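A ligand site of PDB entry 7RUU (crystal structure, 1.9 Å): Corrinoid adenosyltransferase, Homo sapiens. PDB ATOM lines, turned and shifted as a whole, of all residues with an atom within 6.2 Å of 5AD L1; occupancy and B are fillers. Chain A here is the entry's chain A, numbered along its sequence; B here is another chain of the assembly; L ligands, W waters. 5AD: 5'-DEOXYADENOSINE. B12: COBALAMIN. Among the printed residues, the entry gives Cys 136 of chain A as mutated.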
ATOM      1  N   PHE A 116       3.859   7.538 -15.214  1.00  0.00           N
ATOM      2  CA  PHE A 116       3.990   8.865 -15.785  1.00  0.00           C
ATOM      3  C   PHE A 116       4.456   9.838 -14.709  1.00  0.00           C
ATOM      4  O   PHE A 116       4.097   9.715 -13.537  1.00  0.00           O
ATOM      5  CB  PHE A 116       2.645   9.350 -16.361  1.00  0.00           C
ATOM      6  CG  PHE A 116       2.131   8.511 -17.492  1.00  0.00           C
ATOM      7  CD1 PHE A 116       2.804   8.491 -18.695  1.00  0.00           C
ATOM      8  CD2 PHE A 116       0.979   7.737 -17.348  1.00  0.00           C
ATOM      9  CE1 PHE A 116       2.354   7.714 -19.760  1.00  0.00           C
ATOM     10  CE2 PHE A 116       0.528   6.943 -18.402  1.00  0.00           C
ATOM     11  CZ  PHE A 116       1.216   6.941 -19.613  1.00  0.00           C
ATOM     12  N   CYS A 135       8.978  17.397 -30.167  1.00  0.00           N
ATOM     13  CA  CYS A 135       9.635  16.383 -30.993  1.00  0.00           C
ATOM     14  C   CYS A 135       8.619  15.319 -31.402  1.00  0.00           C
ATOM     15  O   CYS A 135       8.632  14.847 -32.546  1.00  0.00           O
ATOM     16  CB  CYS A 135      10.813  15.766 -30.228  1.00  0.00           C
ATOM     17  SG  CYS A 135      11.717  14.431 -31.052  1.00  0.00           S
ATOM     18  N   CYS A 136       7.720  14.931 -30.483  1.00  0.00           N
ATOM     19  CA  CYS A 136       6.640  14.013 -30.855  1.00  0.00           C
ATOM     20  C   CYS A 136       5.738  14.605 -31.933  1.00  0.00           C
ATOM     21  O   CYS A 136       5.281  13.892 -32.844  1.00  0.00           O
ATOM     22  CB  CYS A 136       5.839  13.631 -29.621  1.00  0.00           C
ATOM     23  SG  CYS A 136       6.748  12.451 -28.570  1.00  0.00           S
ATOM     24  N   ARG A 137       5.469  15.913 -31.862  1.00  0.00           N
ATOM     25  CA  ARG A 137       4.692  16.545 -32.924  1.00  0.00           C
ATOM     26  C   ARG A 137       5.425  16.505 -34.265  1.00  0.00           C
ATOM     27  O   ARG A 137       4.824  16.172 -35.298  1.00  0.00           O
ATOM     28  CB  ARG A 137       4.331  17.972 -32.505  1.00  0.00           C
ATOM     29  CG  ARG A 137       3.597  18.792 -33.586  1.00  0.00           C
ATOM     30  CD  ARG A 137       2.634  19.857 -32.966  1.00  0.00           C
ATOM     31  NE  ARG A 137       3.295  20.795 -32.058  1.00  0.00           N
ATOM     32  CZ  ARG A 137       4.044  21.833 -32.455  1.00  0.00           C
ATOM     33  NH1 ARG A 137       4.597  22.634 -31.548  1.00  0.00           N
ATOM     34  NH2 ARG A 137       4.259  22.075 -33.750  1.00  0.00           N
ATOM     35  N   GLU A 139       7.531  14.214 -35.186  1.00  0.00           N
ATOM     36  CA  GLU A 139       7.413  12.829 -35.634  1.00  0.00           C
ATOM     37  C   GLU A 139       6.067  12.565 -36.305  1.00  0.00           C
ATOM     38  O   GLU A 139       6.018  11.914 -37.363  1.00  0.00           O
ATOM     39  CB  GLU A 139       7.619  11.883 -34.440  1.00  0.00           C
ATOM     40  CG  GLU A 139       7.616  10.399 -34.810  1.00  0.00           C
ATOM     41  CD  GLU A 139       7.759   9.490 -33.600  1.00  0.00           C
ATOM     42  OE1 GLU A 139       7.489   9.929 -32.452  1.00  0.00           O
ATOM     43  OE2 GLU A 139       8.140   8.308 -33.782  1.00  0.00           O
ATOM     44  N   ARG A 140       4.969  13.083 -35.733  1.00  0.00           N
ATOM     45  CA  ARG A 140       3.665  12.934 -36.350  1.00  0.00           C
ATOM     46  C   ARG A 140       3.609  13.560 -37.734  1.00  0.00           C
ATOM     47  O   ARG A 140       2.899  13.056 -38.618  1.00  0.00           O
ATOM     48  CB  ARG A 140       2.567  13.546 -35.463  1.00  0.00           C
ATOM     49  CG  ARG A 140       2.341  12.791 -34.153  1.00  0.00           C
ATOM     50  CD  ARG A 140       1.005  13.180 -33.450  1.00  0.00           C
ATOM     51  NE  ARG A 140       0.845  14.626 -33.208  1.00  0.00           N
ATOM     52  CZ  ARG A 140       1.355  15.280 -32.163  1.00  0.00           C
ATOM     53  NH1 ARG A 140       2.115  14.645 -31.256  1.00  0.00           N
ATOM     54  NH2 ARG A 140       1.117  16.586 -32.016  1.00  0.00           N
ATOM     55  N   ASN A 160      11.805   9.497 -33.112  1.00  0.00           N
ATOM     56  CA  ASN A 160      11.265   8.651 -32.046  1.00  0.00           C
ATOM     57  C   ASN A 160      12.298   8.474 -30.938  1.00  0.00           C
ATOM     58  O   ASN A 160      11.965   8.638 -29.760  1.00  0.00           O
ATOM     59  CB  ASN A 160      10.822   7.299 -32.616  1.00  0.00           C
ATOM     60  CG  ASN A 160      10.367   6.331 -31.547  1.00  0.00           C
ATOM     61  OD1 ASN A 160      11.102   5.411 -31.179  1.00  0.00           O
ATOM     62  ND2 ASN A 160       9.166   6.534 -31.030  1.00  0.00           N
ATOM     63  N   VAL B  28      -6.416  10.860 -32.478  1.00  0.00           N
ATOM     64  CA  VAL B  28      -6.168  10.588 -31.063  1.00  0.00           C
ATOM     65  C   VAL B  28      -4.723  10.898 -30.702  1.00  0.00           C
ATOM     66  O   VAL B  28      -4.446  11.510 -29.667  1.00  0.00           O
ATOM     67  CB  VAL B  28      -6.542   9.132 -30.713  1.00  0.00           C
ATOM     68  CG1 VAL B  28      -6.090   8.798 -29.302  1.00  0.00           C
ATOM     69  CG2 VAL B  28      -8.045   8.932 -30.849  1.00  0.00           C
ATOM     70  N   PHE B  29      -3.765  10.476 -31.544  1.00  0.00           N
ATOM     71  CA  PHE B  29      -2.358  10.797 -31.300  1.00  0.00           C
ATOM     72  C   PHE B  29      -2.133  12.304 -31.285  1.00  0.00           C
ATOM     73  O   PHE B  29      -1.364  12.817 -30.456  1.00  0.00           O
ATOM     74  CB  PHE B  29      -1.473  10.154 -32.364  1.00  0.00           C
ATOM     75  CG  PHE B  29      -1.330   8.667 -32.224  1.00  0.00           C
ATOM     76  CD1 PHE B  29      -1.013   8.100 -31.005  1.00  0.00           C
ATOM     77  CD2 PHE B  29      -1.499   7.843 -33.322  1.00  0.00           C
ATOM     78  CE1 PHE B  29      -0.881   6.723 -30.880  1.00  0.00           C
ATOM     79  CE2 PHE B  29      -1.373   6.463 -33.203  1.00  0.00           C
ATOM     80  CZ  PHE B  29      -1.058   5.911 -31.978  1.00  0.00           C
ATOM     81  N   GLU B  30      -2.766  13.029 -32.208  1.00  0.00           N
ATOM     82  CA  GLU B  30      -2.677  14.480 -32.218  1.00  0.00           C
ATOM     83  C   GLU B  30      -3.258  15.080 -30.937  1.00  0.00           C
ATOM     84  O   GLU B  30      -2.684  16.017 -30.372  1.00  0.00           O
ATOM     85  CB  GLU B  30      -3.411  15.047 -33.435  1.00  0.00           C
ATOM     86  CG  GLU B  30      -3.292  16.544 -33.555  1.00  0.00           C
ATOM     87  CD  GLU B  30      -1.901  16.970 -33.946  1.00  0.00           C
ATOM     88  OE1 GLU B  30      -1.140  16.118 -34.455  1.00  0.00           O
ATOM     89  OE2 GLU B  30      -1.573  18.157 -33.754  1.00  0.00           O
ATOM     90  N   VAL B  32      -3.646  13.594 -27.886  1.00  0.00           N
ATOM     91  CA  VAL B  32      -2.884  13.299 -26.669  1.00  0.00           C
ATOM     92  C   VAL B  32      -1.528  13.983 -26.715  1.00  0.00           C
ATOM     93  O   VAL B  32      -1.026  14.437 -25.686  1.00  0.00           O
ATOM     94  CB  VAL B  32      -2.723  11.780 -26.411  1.00  0.00           C
ATOM     95  CG1 VAL B  32      -4.070  11.145 -26.045  1.00  0.00           C
ATOM     96  CG2 VAL B  32      -2.040  11.059 -27.576  1.00  0.00           C
ATOM     97  N   GLY B  33      -0.936  14.097 -27.901  1.00  0.00           N
ATOM     98  CA  GLY B  33       0.324  14.816 -28.031  1.00  0.00           C
ATOM     99  C   GLY B  33       0.198  16.284 -27.659  1.00  0.00           C
ATOM    100  O   GLY B  33       1.068  16.821 -26.971  1.00  0.00           O
HETATM  101  N1  5AD L   1       2.814  11.872 -30.853  1.00  0.00           N
HETATM  102  C2  5AD L   1       1.846  11.530 -29.961  1.00  0.00           C
HETATM  103  N3  5AD L   1       1.562  10.406 -29.270  1.00  0.00           N
HETATM  104  C4  5AD L   1       2.509   9.482 -29.617  1.00  0.00           C
HETATM  105  N9  5AD L   1       2.586   8.150 -29.129  1.00  0.00           N
HETATM  106  C8  5AD L   1       3.726   7.629 -29.777  1.00  0.00           C
HETATM  107  N7  5AD L   1       4.359   8.440 -30.614  1.00  0.00           N
HETATM  108  C5  5AD L   1       3.567   9.620 -30.504  1.00  0.00           C
HETATM  109  C6  5AD L   1       3.704  10.872 -31.137  1.00  0.00           C
HETATM  110  N6  5AD L   1       4.694  11.144 -32.005  1.00  0.00           N
HETATM  111  C1' 5AD L   1       1.685   7.613 -28.148  1.00  0.00           C
HETATM  112  C2' 5AD L   1       1.494   6.036 -28.307  1.00  0.00           C
HETATM  113  C3' 5AD L   1       2.505   5.504 -27.255  1.00  0.00           C
HETATM  114  C4' 5AD L   1       2.420   6.616 -26.191  1.00  0.00           C
HETATM  115  C5' 5AD L   1       3.572   6.553 -25.192  1.00  0.00           C
HETATM  116  O4' 5AD L   1       2.402   7.821 -26.909  1.00  0.00           O
HETATM  117  O2' 5AD L   1       0.219   5.793 -27.935  1.00  0.00           O
HETATM  118  O3' 5AD L   1       2.137   4.269 -26.800  1.00  0.00           O
HETATM  119 CO   B12 L   2       3.147   6.822 -23.228  1.00  0.00          CO
HETATM  120  N21 B12 L   2       4.074   5.280 -22.777  1.00  0.00           N
HETATM  121  N22 B12 L   2       4.744   7.837 -22.885  1.00  0.00           N
HETATM  122  N23 B12 L   2       1.987   8.248 -23.489  1.00  0.00           N
HETATM  123  N24 B12 L   2       1.682   5.606 -23.390  1.00  0.00           N
HETATM  124  C1  B12 L   2       3.294   4.086 -22.404  1.00  0.00           C
HETATM  125  C20 B12 L   2       2.852   4.104 -20.906  1.00  0.00           C
HETATM  126  C2  B12 L   2       4.301   2.889 -22.725  1.00  0.00           C
HETATM  127  C25 B12 L   2       3.983   1.626 -21.865  1.00  0.00           C
HETATM  128  C26 B12 L   2       4.238   2.608 -24.248  1.00  0.00           C
HETATM  129  C27 B12 L   2       5.261   1.551 -24.665  1.00  0.00           C
HETATM  130  O28 B12 L   2       5.133   0.318 -24.709  1.00  0.00           O
HETATM  131  N29 B12 L   2       6.444   2.037 -25.035  1.00  0.00           N
HETATM  132  C3  B12 L   2       5.661   3.581 -22.406  1.00  0.00           C
HETATM  133  C30 B12 L   2       6.268   3.427 -20.945  1.00  0.00           C
HETATM  134  C31 B12 L   2       7.181   2.162 -20.804  1.00  0.00           C
HETATM  135  C32 B12 L   2       8.549   2.374 -21.421  1.00  0.00           C
HETATM  136  O34 B12 L   2       8.822   1.708 -22.421  1.00  0.00           O
HETATM  137  N33 B12 L   2       9.433   3.239 -20.926  1.00  0.00           N
HETATM  138  C4  B12 L   2       5.361   5.031 -22.708  1.00  0.00           C
HETATM  139  C5  B12 L   2       6.392   6.048 -22.855  1.00  0.00           C
HETATM  140  C35 B12 L   2       7.804   5.509 -23.231  1.00  0.00           C
HETATM  141  C6  B12 L   2       6.062   7.392 -22.768  1.00  0.00           C
HETATM  142  C7  B12 L   2       7.010   8.603 -22.861  1.00  0.00           C
HETATM  143  C36 B12 L   2       8.288   8.529 -22.018  1.00  0.00           C
HETATM  144  C37 B12 L   2       7.270   8.869 -24.393  1.00  0.00           C
HETATM  145  C38 B12 L   2       8.250  10.064 -24.674  1.00  0.00           C
HETATM  146  O39 B12 L   2       7.737  11.216 -24.679  1.00  0.00           O
HETATM  147  N40 B12 L   2       9.524   9.797 -24.913  1.00  0.00           N
HETATM  148  C8  B12 L   2       6.036   9.746 -22.379  1.00  0.00           C
HETATM  149  C41 B12 L   2       6.034   9.927 -20.813  1.00  0.00           C
HETATM  150  C42 B12 L   2       5.175  11.150 -20.402  1.00  0.00           C
HETATM  151  C43 B12 L   2       5.276  11.510 -18.957  1.00  0.00           C
HETATM  152  O44 B12 L   2       5.714  10.678 -18.124  1.00  0.00           O
HETATM  153  N45 B12 L   2       4.929  12.729 -18.511  1.00  0.00           N
HETATM  154  C9  B12 L   2       4.680   9.171 -22.756  1.00  0.00           C
HETATM  155  C10 B12 L   2       3.647   9.988 -23.160  1.00  0.00           C
HETATM  156  C11 B12 L   2       2.374   9.572 -23.486  1.00  0.00           C
HETATM  157  C12 B12 L   2       1.274  10.527 -23.959  1.00  0.00           C
HETATM  158  C46 B12 L   2       1.535  10.845 -25.465  1.00  0.00           C
HETATM  159  C47 B12 L   2       1.217  11.899 -23.229  1.00  0.00           C
HETATM  160  C13 B12 L   2       0.013   9.628 -23.850  1.00  0.00           C
HETATM  161  C48 B12 L   2      -0.887  10.027 -22.613  1.00  0.00           C
HETATM  162  C49 B12 L   2      -0.302   9.488 -21.290  1.00  0.00           C
HETATM  163  C50 B12 L   2      -1.250   9.933 -20.170  1.00  0.00           C
HETATM  164  O51 B12 L   2      -2.195   9.124 -19.876  1.00  0.00           O
HETATM  165  N52 B12 L   2      -1.082  11.063 -19.597  1.00  0.00           N
HETATM  166  C14 B12 L   2       0.594   8.242 -23.704  1.00  0.00           C
HETATM  167  C15 B12 L   2      -0.213   7.118 -23.837  1.00  0.00           C
HETATM  168  C53 B12 L   2      -1.682   7.306 -24.219  1.00  0.00           C
HETATM  169  C16 B12 L   2       0.424   5.841 -23.589  1.00  0.00           C
HETATM  170  C17 B12 L   2      -0.304   4.470 -23.339  1.00  0.00           C
HETATM  171  C54 B12 L   2      -0.543   4.175 -24.880  1.00  0.00           C
HETATM  172  C55 B12 L   2      -1.600   4.397 -22.593  1.00  0.00           C
HETATM  173  C56 B12 L   2      -1.416   5.184 -21.273  1.00  0.00           C
HETATM  174  C57 B12 L   2      -2.730   5.186 -20.485  1.00  0.00           C
HETATM  175  O58 B12 L   2      -3.686   5.815 -20.897  1.00  0.00           O
HETATM  176  N59 B12 L   2      -2.731   4.481 -19.377  1.00  0.00           N
HETATM  177  C18 B12 L   2       0.765   3.496 -22.843  1.00  0.00           C
HETATM  178  C60 B12 L   2       0.675   2.008 -23.339  1.00  0.00           C
HETATM  179  C61 B12 L   2      -0.557   1.279 -22.813  1.00  0.00           C
HETATM  180  O63 B12 L   2      -0.790   1.215 -21.595  1.00  0.00           O
HETATM  181  N62 B12 L   2      -1.373   0.771 -23.748  1.00  0.00           N
HETATM  182  C19 B12 L   2       2.025   4.187 -23.314  1.00  0.00           C
HETATM  183  C1P B12 L   2      -3.981   4.507 -18.601  1.00  0.00           C
HETATM  184  C2P B12 L   2      -3.593   5.034 -17.207  1.00  0.00           C
HETATM  185  C3P B12 L   2      -4.796   5.134 -16.256  1.00  0.00           C
HETATM  186  O3  B12 L   2      -2.642   4.044 -16.690  1.00  0.00           O
HETATM  187  O4  B12 L   2      -2.474   3.794 -14.150  1.00  0.00           O
HETATM  188  O5  B12 L   2      -1.158   5.662 -15.340  1.00  0.00           O
HETATM  189  P   B12 L   2      -1.756   4.243 -15.341  1.00  0.00           P
HETATM  190  O2  B12 L   2      -0.528   3.218 -15.618  1.00  0.00           O
HETATM  191  C3R B12 L   2       0.366   3.426 -16.669  1.00  0.00           C
HETATM  192  C2R B12 L   2       1.782   3.695 -16.245  1.00  0.00           C
HETATM  193  O7R B12 L   2       2.172   2.888 -15.172  1.00  0.00           O
HETATM  194  C1R B12 L   2       2.540   3.303 -17.540  1.00  0.00           C
HETATM  195  O6R B12 L   2       1.871   2.133 -17.974  1.00  0.00           O
HETATM  196  C4R B12 L   2       0.567   2.031 -17.347  1.00  0.00           C
HETATM  197  C5R B12 L   2      -0.525   1.602 -18.330  1.00  0.00           C
HETATM  198  O8R B12 L   2      -0.701   2.617 -19.376  1.00  0.00           O
HETATM  199  N1B B12 L   2       3.954   2.929 -17.416  1.00  0.00           N
HETATM  200  C8B B12 L   2       5.054   3.770 -17.571  1.00  0.00           C
HETATM  201  C2B B12 L   2       4.433   1.703 -17.139  1.00  0.00           C
HETATM  202  N3B B12 L   2       5.757   1.678 -17.106  1.00  0.00           N
HETATM  203  C9B B12 L   2       6.179   2.983 -17.391  1.00  0.00           C
HETATM  204  C4B B12 L   2       7.462   3.559 -17.483  1.00  0.00           C
HETATM  205  C5B B12 L   2       7.524   4.933 -17.782  1.00  0.00           C
HETATM  206  C5M B12 L   2       8.866   5.620 -17.918  1.00  0.00           C
HETATM  207  C6B B12 L   2       6.336   5.745 -17.983  1.00  0.00           C
HETATM  208  C6M B12 L   2       6.453   7.213 -18.298  1.00  0.00           C
HETATM  209  C7B B12 L   2       5.058   5.148 -17.868  1.00  0.00           C
HETATM  210  O   HOH W   1       4.841   9.387 -27.105  1.00  0.00           O
HETATM  211  O   HOH W   2      -1.429   3.531 -28.392  1.00  0.00           O
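A nitrogen (N1) of 5AD L1 lies within hydrogen-bond range of the guanidinium group of Arg 140 (2.9 Å). N6 of 5AD L1 sits at hydrogen-bond distance from O of Cys 136 (2.9 Å). The side-chain carboxylate (OE1) of Glu 139 sits at hydrogen-bond distance from a nitrogen (N6) of 5AD L1 (3.1 Å).
The guanidinium group (NE) of Arg 140 is in salt-bridge range of the side-chain carboxylate (OE1) of Glu 30 of chain B (2.8 Å). The side-chain amide nitrogen of Asn 160 lies close to the side-chain carboxylate of Glu 139, at 3.4 Å.
Residues that only touch 5AD L1: Phe 29 of chain B. Hydrophobic or aromatic side chains that line 5AD L1: Phe 29 of chain B. Within 4 Å of 5AD L1: Cys 136, Glu 139, Arg 140 and Phe 29 of chain B.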
